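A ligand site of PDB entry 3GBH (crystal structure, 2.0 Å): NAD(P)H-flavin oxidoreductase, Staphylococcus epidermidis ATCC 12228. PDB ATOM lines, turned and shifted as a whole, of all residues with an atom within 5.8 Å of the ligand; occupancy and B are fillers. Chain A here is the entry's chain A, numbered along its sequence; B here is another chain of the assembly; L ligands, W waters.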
ATOM      1  N   ARG A  18     -11.595 -29.966   8.390  1.00  0.00           N
ATOM      2  CA  ARG A  18     -12.541 -29.346   7.446  1.00  0.00           C
ATOM      3  C   ARG A  18     -11.872 -29.362   6.079  1.00  0.00           C
ATOM      4  O   ARG A  18     -10.964 -28.576   5.825  1.00  0.00           O
ATOM      5  CB  ARG A  18     -12.861 -27.914   7.899  1.00  0.00           C
ATOM      6  CG  ARG A  18     -14.117 -27.202   7.353  1.00  0.00           C
ATOM      7  CD  ARG A  18     -14.137 -26.929   5.859  1.00  0.00           C
ATOM      8  NE  ARG A  18     -12.916 -26.285   5.397  1.00  0.00           N
ATOM      9  CZ  ARG A  18     -12.410 -26.419   4.178  1.00  0.00           C
ATOM     10  NH1 ARG A  18     -13.024 -27.159   3.266  1.00  0.00           N
ATOM     11  NH2 ARG A  18     -11.271 -25.803   3.868  1.00  0.00           N
ATOM     12  N   LYS A  19     -12.314 -30.283   5.227  1.00  0.00           N
ATOM     13  CA  LYS A  19     -11.787 -30.425   3.873  1.00  0.00           C
ATOM     14  C   LYS A  19     -12.961 -30.705   2.938  1.00  0.00           C
ATOM     15  O   LYS A  19     -14.012 -31.094   3.398  1.00  0.00           O
ATOM     16  CB  LYS A  19     -10.780 -31.577   3.816  1.00  0.00           C
ATOM     17  CG  LYS A  19      -9.509 -31.321   4.661  1.00  0.00           C
ATOM     18  CD  LYS A  19      -8.577 -32.497   4.670  1.00  0.00           C
ATOM     19  CE  LYS A  19      -7.335 -32.267   5.550  1.00  0.00           C
ATOM     20  NZ  LYS A  19      -6.506 -33.548   5.628  1.00  0.00           N
ATOM     21  N   SER A  20     -12.793 -30.432   1.646  1.00  0.00           N
ATOM     22  CA  SER A  20     -13.850 -30.644   0.651  1.00  0.00           C
ATOM     23  C   SER A  20     -13.996 -32.122   0.341  1.00  0.00           C
ATOM     24  O   SER A  20     -13.177 -32.708  -0.359  1.00  0.00           O
ATOM     25  CB  SER A  20     -13.554 -29.837  -0.615  1.00  0.00           C
ATOM     26  OG  SER A  20     -13.715 -28.442  -0.383  1.00  0.00           O
ATOM     27  N   LYS A  22     -16.060 -34.911  -1.584  1.00  0.00           N
ATOM     28  CA  LYS A  22     -16.889 -34.886  -2.785  1.00  0.00           C
ATOM     29  C   LYS A  22     -17.710 -36.130  -2.991  1.00  0.00           C
ATOM     30  O   LYS A  22     -18.643 -36.090  -3.787  1.00  0.00           O
ATOM     31  CB  LYS A  22     -16.047 -34.547  -4.002  1.00  0.00           C
ATOM     32  CG  LYS A  22     -15.358 -33.196  -3.779  1.00  0.00           C
ATOM     33  CD  LYS A  22     -14.627 -32.629  -4.970  1.00  0.00           C
ATOM     34  CE  LYS A  22     -14.018 -31.262  -4.571  1.00  0.00           C
ATOM     35  NZ  LYS A  22     -13.695 -30.467  -5.771  1.00  0.00           N
ATOM     36  N   ASN A  75     -20.715 -30.889 -10.794  1.00  0.00           N
ATOM     37  CA  ASN A  75     -20.765 -31.266  -9.390  1.00  0.00           C
ATOM     38  C   ASN A  75     -21.815 -32.339  -9.090  1.00  0.00           C
ATOM     39  O   ASN A  75     -22.423 -32.362  -8.001  1.00  0.00           O
ATOM     40  CB  ASN A  75     -20.957 -30.044  -8.523  1.00  0.00           C
ATOM     41  CG  ASN A  75     -19.777 -29.113  -8.590  1.00  0.00           C
ATOM     42  OD1 ASN A  75     -18.694 -29.466  -8.150  1.00  0.00           O
ATOM     43  ND2 ASN A  75     -19.972 -27.948  -9.164  1.00  0.00           N
ATOM     44  N   GLN A  78     -21.375 -34.776  -5.919  1.00  0.00           N
ATOM     45  CA  GLN A  78     -21.779 -34.173  -4.640  1.00  0.00           C
ATOM     46  C   GLN A  78     -23.307 -34.071  -4.525  1.00  0.00           C
ATOM     47  O   GLN A  78     -23.895 -34.436  -3.500  1.00  0.00           O
ATOM     48  CB  GLN A  78     -21.137 -32.788  -4.415  1.00  0.00           C
ATOM     49  CG  GLN A  78     -19.609 -32.751  -4.526  1.00  0.00           C
ATOM     50  CD  GLN A  78     -19.126 -32.334  -5.905  1.00  0.00           C
ATOM     51  OE1 GLN A  78     -19.449 -32.992  -6.890  1.00  0.00           O
ATOM     52  NE2 GLN A  78     -18.381 -31.226  -5.998  1.00  0.00           N
ATOM     53  N   ASN A 162     -18.687 -29.811   1.212  1.00  0.00           N
ATOM     54  CA  ASN A 162     -17.958 -29.279   0.064  1.00  0.00           C
ATOM     55  C   ASN A 162     -18.704 -28.005  -0.381  1.00  0.00           C
ATOM     56  O   ASN A 162     -19.866 -28.064  -0.761  1.00  0.00           O
ATOM     57  CB  ASN A 162     -17.958 -30.319  -1.060  1.00  0.00           C
ATOM     58  CG  ASN A 162     -17.363 -29.811  -2.374  1.00  0.00           C
ATOM     59  OD1 ASN A 162     -17.782 -30.241  -3.425  1.00  0.00           O
ATOM     60  ND2 ASN A 162     -16.403 -28.889  -2.306  1.00  0.00           N
ATOM     61  N   PRO A 163     -18.039 -26.839  -0.311  1.00  0.00           N
ATOM     62  CA  PRO A 163     -18.627 -25.623  -0.792  1.00  0.00           C
ATOM     63  C   PRO A 163     -18.531 -25.575  -2.289  1.00  0.00           C
ATOM     64  O   PRO A 163     -17.541 -25.994  -2.844  1.00  0.00           O
ATOM     65  CB  PRO A 163     -17.772 -24.537  -0.153  1.00  0.00           C
ATOM     66  CG  PRO A 163     -16.428 -25.128  -0.050  1.00  0.00           C
ATOM     67  CD  PRO A 163     -16.687 -26.606   0.233  1.00  0.00           C
ATOM     68  N   ILE A 164     -19.588 -25.099  -2.938  1.00  0.00           N
ATOM     69  CA  ILE A 164     -19.763 -25.256  -4.387  1.00  0.00           C
ATOM     70  C   ILE A 164     -20.276 -23.932  -4.961  1.00  0.00           C
ATOM     71  O   ILE A 164     -21.299 -23.397  -4.522  1.00  0.00           O
ATOM     72  CB  ILE A 164     -20.744 -26.435  -4.735  1.00  0.00           C
ATOM     73  CG1 ILE A 164     -20.115 -27.795  -4.460  1.00  0.00           C
ATOM     74  CG2 ILE A 164     -21.236 -26.386  -6.219  1.00  0.00           C
ATOM     75  CD1 ILE A 164     -21.152 -28.942  -4.365  1.00  0.00           C
ATOM     76  N   GLY A 165     -19.519 -23.385  -5.894  1.00  0.00           N
ATOM     77  CA  GLY A 165     -19.922 -22.182  -6.616  1.00  0.00           C
ATOM     78  C   GLY A 165     -20.279 -22.476  -8.042  1.00  0.00           C
ATOM     79  O   GLY A 165     -20.870 -21.635  -8.742  1.00  0.00           O
ATOM     80  N   GLY A 166     -19.932 -23.672  -8.509  1.00  0.00           N
ATOM     81  CA  GLY A 166     -20.127 -24.013  -9.919  1.00  0.00           C
ATOM     82  C   GLY A 166     -21.517 -24.555 -10.181  1.00  0.00           C
ATOM     83  O   GLY A 166     -21.673 -25.715 -10.566  1.00  0.00           O
ATOM     84  N   PHE A 167     -22.538 -23.729  -9.946  1.00  0.00           N
ATOM     85  CA  PHE A 167     -23.905 -24.096 -10.315  1.00  0.00           C
ATOM     86  C   PHE A 167     -24.582 -22.939 -11.059  1.00  0.00           C
ATOM     87  O   PHE A 167     -24.089 -21.814 -11.027  1.00  0.00           O
ATOM     88  CB  PHE A 167     -24.691 -24.568  -9.086  1.00  0.00           C
ATOM     89  CG  PHE A 167     -24.841 -23.550  -7.985  1.00  0.00           C
ATOM     90  CD1 PHE A 167     -23.799 -23.254  -7.131  1.00  0.00           C
ATOM     91  CD2 PHE A 167     -26.079 -22.945  -7.746  1.00  0.00           C
ATOM     92  CE1 PHE A 167     -23.945 -22.347  -6.106  1.00  0.00           C
ATOM     93  CE2 PHE A 167     -26.239 -22.031  -6.710  1.00  0.00           C
ATOM     94  CZ  PHE A 167     -25.183 -21.720  -5.904  1.00  0.00           C
ATOM     95  N   LEU A 187     -23.851 -19.261  -2.413  1.00  0.00           N
ATOM     96  CA  LEU A 187     -23.083 -20.494  -2.551  1.00  0.00           C
ATOM     97  C   LEU A 187     -23.909 -21.685  -2.093  1.00  0.00           C
ATOM     98  O   LEU A 187     -24.941 -21.539  -1.441  1.00  0.00           O
ATOM     99  CB  LEU A 187     -21.726 -20.417  -1.804  1.00  0.00           C
ATOM    100  CG  LEU A 187     -21.699 -20.516  -0.265  1.00  0.00           C
ATOM    101  CD1 LEU A 187     -20.298 -20.930   0.229  1.00  0.00           C
ATOM    102  CD2 LEU A 187     -22.104 -19.237   0.393  1.00  0.00           C
ATOM    103  N   ALA A 198     -11.225 -36.636   1.543  1.00  0.00           N
ATOM    104  CA  ALA A 198     -10.865 -35.483   0.734  1.00  0.00           C
ATOM    105  C   ALA A 198      -9.401 -35.565   0.328  1.00  0.00           C
ATOM    106  O   ALA A 198      -8.579 -36.113   1.046  1.00  0.00           O
ATOM    107  CB  ALA A 198     -11.101 -34.207   1.516  1.00  0.00           C
ATOM    108  N   HIS A 199      -9.084 -35.024  -0.852  1.00  0.00           N
ATOM    109  CA  HIS A 199      -7.692 -34.807  -1.233  1.00  0.00           C
ATOM    110  C   HIS A 199      -7.202 -33.633  -0.419  1.00  0.00           C
ATOM    111  O   HIS A 199      -7.937 -32.675  -0.191  1.00  0.00           O
ATOM    112  CB  HIS A 199      -7.563 -34.422  -2.702  1.00  0.00           C
ATOM    113  CG  HIS A 199      -7.968 -35.500  -3.644  1.00  0.00           C
ATOM    114  ND1 HIS A 199      -7.051 -36.352  -4.227  1.00  0.00           N
ATOM    115  CD2 HIS A 199      -9.186 -35.881  -4.094  1.00  0.00           C
ATOM    116  CE1 HIS A 199      -7.691 -37.206  -5.009  1.00  0.00           C
ATOM    117  NE2 HIS A 199      -8.990 -36.944  -4.947  1.00  0.00           N
ATOM    118  N   SER A 201      -4.986 -30.256   0.117  1.00  0.00           N
ATOM    119  CA  SER A 201      -4.730 -29.117  -0.731  1.00  0.00           C
ATOM    120  C   SER A 201      -3.701 -28.202  -0.076  1.00  0.00           C
ATOM    121  O   SER A 201      -3.515 -28.248   1.135  1.00  0.00           O
ATOM    122  CB  SER A 201      -6.010 -28.366  -1.002  1.00  0.00           C
ATOM    123  OG  SER A 201      -6.553 -27.928   0.231  1.00  0.00           O
ATOM    124  N   ARG A 203      -1.758 -24.394   0.666  1.00  0.00           N
ATOM    125  CA  ARG A 203      -2.024 -22.982   0.890  1.00  0.00           C
ATOM    126  C   ARG A 203      -0.741 -22.209   0.694  1.00  0.00           C
ATOM    127  O   ARG A 203       0.333 -22.721   0.927  1.00  0.00           O
ATOM    128  CB  ARG A 203      -2.589 -22.729   2.273  1.00  0.00           C
ATOM    129  CG  ARG A 203      -3.947 -23.408   2.517  1.00  0.00           C
ATOM    130  CD  ARG A 203      -5.056 -22.703   1.712  1.00  0.00           C
ATOM    131  NE  ARG A 203      -6.371 -23.263   2.017  1.00  0.00           N
ATOM    132  CZ  ARG A 203      -6.813 -24.451   1.576  1.00  0.00           C
ATOM    133  NH1 ARG A 203      -6.055 -25.203   0.810  1.00  0.00           N
ATOM    134  NH2 ARG A 203      -8.019 -24.891   1.939  1.00  0.00           N
ATOM    135  N   LYS B  44      -6.488 -21.587   5.986  1.00  0.00           N
ATOM    136  CA  LYS B  44      -6.948 -22.972   5.675  1.00  0.00           C
ATOM    137  C   LYS B  44      -8.391 -23.023   5.184  1.00  0.00           C
ATOM    138  O   LYS B  44      -8.872 -24.075   4.774  1.00  0.00           O
ATOM    139  CB  LYS B  44      -6.783 -23.904   6.889  1.00  0.00           C
ATOM    140  CG  LYS B  44      -5.357 -24.217   7.209  1.00  0.00           C
ATOM    141  CD  LYS B  44      -5.168 -25.065   8.521  1.00  0.00           C
ATOM    142  CE  LYS B  44      -5.612 -26.504   8.330  1.00  0.00           C
ATOM    143  NZ  LYS B  44      -4.749 -27.189   7.338  1.00  0.00           N
ATOM    144  N   ALA B  45      -9.090 -21.895   5.235  1.00  0.00           N
ATOM    145  CA  ALA B  45     -10.418 -21.743   4.651  1.00  0.00           C
ATOM    146  C   ALA B  45     -10.411 -22.172   3.195  1.00  0.00           C
ATOM    147  O   ALA B  45      -9.384 -22.038   2.505  1.00  0.00           O
ATOM    148  CB  ALA B  45     -10.844 -20.266   4.735  1.00  0.00           C
ATOM    149  N   PRO B  46     -11.552 -22.635   2.691  1.00  0.00           N
ATOM    150  CA  PRO B  46     -11.626 -22.994   1.294  1.00  0.00           C
ATOM    151  C   PRO B  46     -11.811 -21.752   0.430  1.00  0.00           C
ATOM    152  O   PRO B  46     -12.222 -20.702   0.903  1.00  0.00           O
ATOM    153  CB  PRO B  46     -12.892 -23.868   1.234  1.00  0.00           C
ATOM    154  CG  PRO B  46     -13.761 -23.295   2.287  1.00  0.00           C
ATOM    155  CD  PRO B  46     -12.853 -22.803   3.365  1.00  0.00           C
ATOM    156  N   SER B  47     -11.509 -21.897  -0.857  1.00  0.00           N
ATOM    157  CA  SER B  47     -11.750 -20.833  -1.808  1.00  0.00           C
ATOM    158  C   SER B  47     -11.982 -21.437  -3.178  1.00  0.00           C
ATOM    159  O   SER B  47     -11.580 -22.569  -3.450  1.00  0.00           O
ATOM    160  CB  SER B  47     -10.560 -19.874  -1.864  1.00  0.00           C
ATOM    161  OG  SER B  47      -9.389 -20.558  -2.301  1.00  0.00           O
ATOM    162  N   SER B  48     -12.632 -20.665  -4.038  1.00  0.00           N
ATOM    163  CA  SER B  48     -12.983 -21.139  -5.372  1.00  0.00           C
ATOM    164  C   SER B  48     -11.680 -21.521  -6.086  1.00  0.00           C
ATOM    165  O   SER B  48     -10.730 -20.739  -6.092  1.00  0.00           O
ATOM    166  CB  SER B  48     -13.807 -20.050  -6.118  1.00  0.00           C
ATOM    167  OG  SER B  48     -14.100 -20.428  -7.447  1.00  0.00           O
ATOM    168  N   VAL B  49     -11.639 -22.717  -6.657  1.00  0.00           N
ATOM    169  CA  VAL B  49     -10.439 -23.325  -7.282  1.00  0.00           C
ATOM    170  C   VAL B  49      -9.133 -23.158  -6.488  1.00  0.00           C
ATOM    171  O   VAL B  49      -8.048 -23.158  -7.069  1.00  0.00           O
ATOM    172  CB  VAL B  49     -10.282 -22.940  -8.787  1.00  0.00           C
ATOM    173  CG1 VAL B  49     -11.417 -23.628  -9.576  1.00  0.00           C
ATOM    174  CG2 VAL B  49     -10.303 -21.450  -8.997  1.00  0.00           C
ATOM    175  N   ASN B  50      -9.270 -23.082  -5.162  1.00  0.00           N
ATOM    176  CA  ASN B  50      -8.143 -22.885  -4.265  1.00  0.00           C
ATOM    177  C   ASN B  50      -7.267 -21.685  -4.604  1.00  0.00           C
ATOM    178  O   ASN B  50      -6.063 -21.692  -4.339  1.00  0.00           O
ATOM    179  CB  ASN B  50      -7.315 -24.167  -4.187  1.00  0.00           C
ATOM    180  CG  ASN B  50      -6.449 -24.220  -2.932  1.00  0.00           C
ATOM    181  OD1 ASN B  50      -6.811 -23.695  -1.872  1.00  0.00           O
ATOM    182  ND2 ASN B  50      -5.287 -24.859  -3.061  1.00  0.00           N
ATOM    183  N   ILE B 141     -16.860 -13.486  -1.507  1.00  0.00           N
ATOM    184  CA  ILE B 141     -17.243 -14.748  -0.907  1.00  0.00           C
ATOM    185  C   ILE B 141     -16.032 -15.446  -0.286  1.00  0.00           C
ATOM    186  O   ILE B 141     -16.069 -15.801   0.894  1.00  0.00           O
ATOM    187  CB  ILE B 141     -18.008 -15.688  -1.891  1.00  0.00           C
ATOM    188  CG1 ILE B 141     -19.367 -15.064  -2.285  1.00  0.00           C
ATOM    189  CG2 ILE B 141     -18.186 -17.069  -1.271  1.00  0.00           C
ATOM    190  CD1 ILE B 141     -19.994 -15.670  -3.542  1.00  0.00           C
ATOM    191  N   ASP B 142     -14.954 -15.621  -1.059  1.00  0.00           N
ATOM    192  CA  ASP B 142     -13.814 -16.389  -0.557  1.00  0.00           C
ATOM    193  C   ASP B 142     -13.244 -15.693   0.665  1.00  0.00           C
ATOM    194  O   ASP B 142     -12.938 -16.344   1.648  1.00  0.00           O
ATOM    195  CB  ASP B 142     -12.712 -16.541  -1.595  1.00  0.00           C
ATOM    196  CG  ASP B 142     -13.069 -17.489  -2.739  1.00  0.00           C
ATOM    197  OD1 ASP B 142     -13.926 -18.380  -2.576  1.00  0.00           O
ATOM    198  OD2 ASP B 142     -12.433 -17.349  -3.823  1.00  0.00           O
ATOM    199  N   LEU B 145     -15.261 -16.135   3.804  1.00  0.00           N
ATOM    200  CA  LEU B 145     -15.071 -17.451   4.394  1.00  0.00           C
ATOM    201  C   LEU B 145     -13.839 -17.450   5.308  1.00  0.00           C
ATOM    202  O   LEU B 145     -13.886 -17.950   6.436  1.00  0.00           O
ATOM    203  CB  LEU B 145     -14.969 -18.542   3.320  1.00  0.00           C
ATOM    204  CG  LEU B 145     -16.195 -18.793   2.422  1.00  0.00           C
ATOM    205  CD1 LEU B 145     -15.856 -19.790   1.340  1.00  0.00           C
ATOM    206  CD2 LEU B 145     -17.396 -19.278   3.256  1.00  0.00           C
HETATM  207  N1  LIG L   1     -15.420 -27.614  -5.458  1.00  0.00           N
HETATM  208  C1  LIG L   1     -16.072 -28.333  -6.439  1.00  0.00           C
HETATM  209  O1  LIG L   1     -15.834 -29.548  -6.554  1.00  0.00           O
HETATM  210  N2  LIG L   1     -16.975 -27.695  -7.281  1.00  0.00           N
HETATM  211  C2  LIG L   1     -17.250 -26.341  -7.157  1.00  0.00           C
HETATM  212  O2  LIG L   1     -18.076 -25.839  -7.936  1.00  0.00           O
HETATM  213  C3  LIG L   1     -16.574 -25.590  -6.168  1.00  0.00           C
HETATM  214  N3  LIG L   1     -16.772 -24.223  -6.021  1.00  0.00           N
HETATM  215  C4  LIG L   1     -16.330 -23.594  -4.869  1.00  0.00           C
HETATM  216  C5  LIG L   1     -16.789 -22.319  -4.543  1.00  0.00           C
HETATM  217  C6  LIG L   1     -16.385 -21.671  -3.401  1.00  0.00           C
HETATM  218  C7  LIG L   1     -16.907 -20.300  -3.069  1.00  0.00           C
HETATM  219  C8  LIG L   1     -15.503 -22.309  -2.551  1.00  0.00           C
HETATM  220  C9  LIG L   1     -15.083 -21.613  -1.292  1.00  0.00           C
HETATM  221  C10 LIG L   1     -15.030 -23.578  -2.842  1.00  0.00           C
HETATM  222  C11 LIG L   1     -15.437 -24.240  -4.015  1.00  0.00           C
HETATM  223  N4  LIG L   1     -14.984 -25.523  -4.343  1.00  0.00           N
HETATM  224  C12 LIG L   1     -15.648 -26.233  -5.326  1.00  0.00           C
HETATM  225  C13 LIG L   1     -14.049 -26.273  -3.406  1.00  0.00           C
HETATM  226  C14 LIG L   1     -12.642 -25.726  -3.573  1.00  0.00           C
HETATM  227  O3  LIG L   1     -11.997 -26.303  -4.707  1.00  0.00           O
HETATM  228  C15 LIG L   1     -11.822 -26.095  -2.341  1.00  0.00           C
HETATM  229  O4  LIG L   1     -12.396 -25.496  -1.201  1.00  0.00           O
HETATM  230  C16 LIG L   1     -10.357 -25.716  -2.467  1.00  0.00           C
HETATM  231  O5  LIG L   1      -9.840 -26.542  -3.492  1.00  0.00           O
HETATM  232  C17 LIG L   1      -9.650 -25.938  -1.131  1.00  0.00           C
HETATM  233  O6  LIG L   1      -9.699 -27.323  -0.725  1.00  0.00           O
HETATM  234  P1  LIG L   1     -10.354 -27.722   0.685  1.00  0.00           P
HETATM  235  O7  LIG L   1     -10.337 -29.242   0.820  1.00  0.00           O
HETATM  236  O8  LIG L   1     -11.774 -27.213   0.727  1.00  0.00           O
HETATM  237  O9  LIG L   1      -9.646 -27.099   1.834  1.00  0.00           O
HETATM  238  O   HOH W   1     -11.623 -28.902  -5.379  1.00  0.00           O
HETATM  239  O   HOH W   2      -9.599 -30.896  -1.412  1.00  0.00           O
HETATM  240  O   HOH W   3     -15.890 -17.473  -4.193  1.00  0.00           O
HETATM  241  O   HOH W   4      -7.864 -30.123   1.377  1.00  0.00           O
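The side-chain amino group of Lys 22 is in hydrogen-bond range of an oxygen (O1) of the ligand (2.5 Å).
An oxygen (O7) of the ligand is in hydrogen-bond range of the backbone NH (N) of Ser 20.
An oxygen (O8) of the ligand is in hydrogen-bond range of the side-chain hydroxyl of Ser 20 (2.6 Å).
A nitrogen (N2) of the ligand sits at hydrogen-bond distance from the side-chain amide oxygen (OD1) of Asn 75 (2.6 Å).
The guanidinium group of Arg 203 is in salt-bridge range of an oxygen (O9) of the ligand, at 2.7 Å.
NH1 of Arg 18 lies within salt-bridge range of O8 of the ligand (2.8 Å).
A nitrogen (N3) of the ligand is in hydrogen-bond range of the backbone NH (N) of Gly 165 (2.9 Å).
The backbone NH of Gly 166 is in hydrogen-bond range of an oxygen (O2) of the ligand (2.9 Å).
An oxygen (O1) of the ligand lies within hydrogen-bond range of the side-chain amide nitrogen (NE2) of Gln 78 (3.1 Å).
An oxygen (O6) of the ligand is in hydrogen-bond range of the side-chain hydroxyl (OG) of Ser 201 (3.3 Å).
ND2 of Asn 162 lies within hydrogen-bond range of OG of Ser 20 (3.3 Å).
ND2 of Asn 75 is in hydrogen-bond range of O of Gly 166.
OD1 of Asn 75 is in hydrogen-bond range of NE2 of Gln 78 (2.8 Å).
OG of Ser 201 lies within hydrogen-bond range of NH1 of Arg 203, 2.8 Å away.
The side-chain amide oxygen (OD1) of Asn 50 of chain B sits at hydrogen-bond distance from the guanidinium group (NH1) of Arg 203 (3.2 Å).
NH2 of Arg 203 is in hydrogen-bond range of O of Lys 44 of chain B (3.1 Å).
The backbone carbonyl oxygen of Ala 45 of chain B is in hydrogen-bond range of the guanidinium group of Arg 203 (3.2 Å).
The backbone carbonyl oxygen of Lys 44 of chain B lies within hydrogen-bond range of the guanidinium group of Arg 18, at 3.1 Å.
N4 of the ligand lies close to O of Pro 163 (3.0 Å).
CA of Lys 19 touches O7 of the ligand, at 3.6 Å.
ND2 of Asn 162 touches N1 of the ligand, at 3.5 Å.
CA of Ile 164 touches N3 of the ligand (3.6 Å).
CB of Pro 46 of chain B touches O4 of the ligand (3.0 Å).
Ser 47 of chain B touches the ligand.
Ser 48 of chain B touches the ligand.
Asn 50 of chain B touches the ligand (CB to O5, 3.5 Å).
Ile 141 of chain B touches the ligand.
OD1 of Asp 142 of chain B touches C7 of the ligand, at 3.6 Å.
Leu 145 of chain B touches the ligand.
Hydrophobic or aromatic side chains within 4 Å of the ligand: Pro 163, Ile 164, Pro 46 of chain B, Ile 141 of chain B and Leu 145 of chain B.
Within 4 Å of the ligand: Arg 18, Lys 19, Ser 20, Lys 22, Asn 75, Gln 78, Asn 162, Pro 163, Ile 164, Gly 165, Gly 166, Ser 201, Arg 203, Pro 46 of chain B, Ser 47 of chain B, Ser 48 of chain B, Asn 50 of chain B, Ile 141 of chain B, Asp 142 of chain B and Leu 145 of chain B.
Water W4 lies within hydrogen-bond range of an oxygen (O7) of the ligand, the side-chain hydroxyl of Ser 201 and the backbone carbonyl oxygen of His 199.
Water W1 lies within hydrogen-bond range of the side-chain amino group (NZ) of Lys 22 (2.6 Å) and an oxygen (O3) of the ligand (2.7 Å).
Water W2 lies within hydrogen-bond range of O of His 199 (2.7 Å) and O7 of the ligand (2.9 Å).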
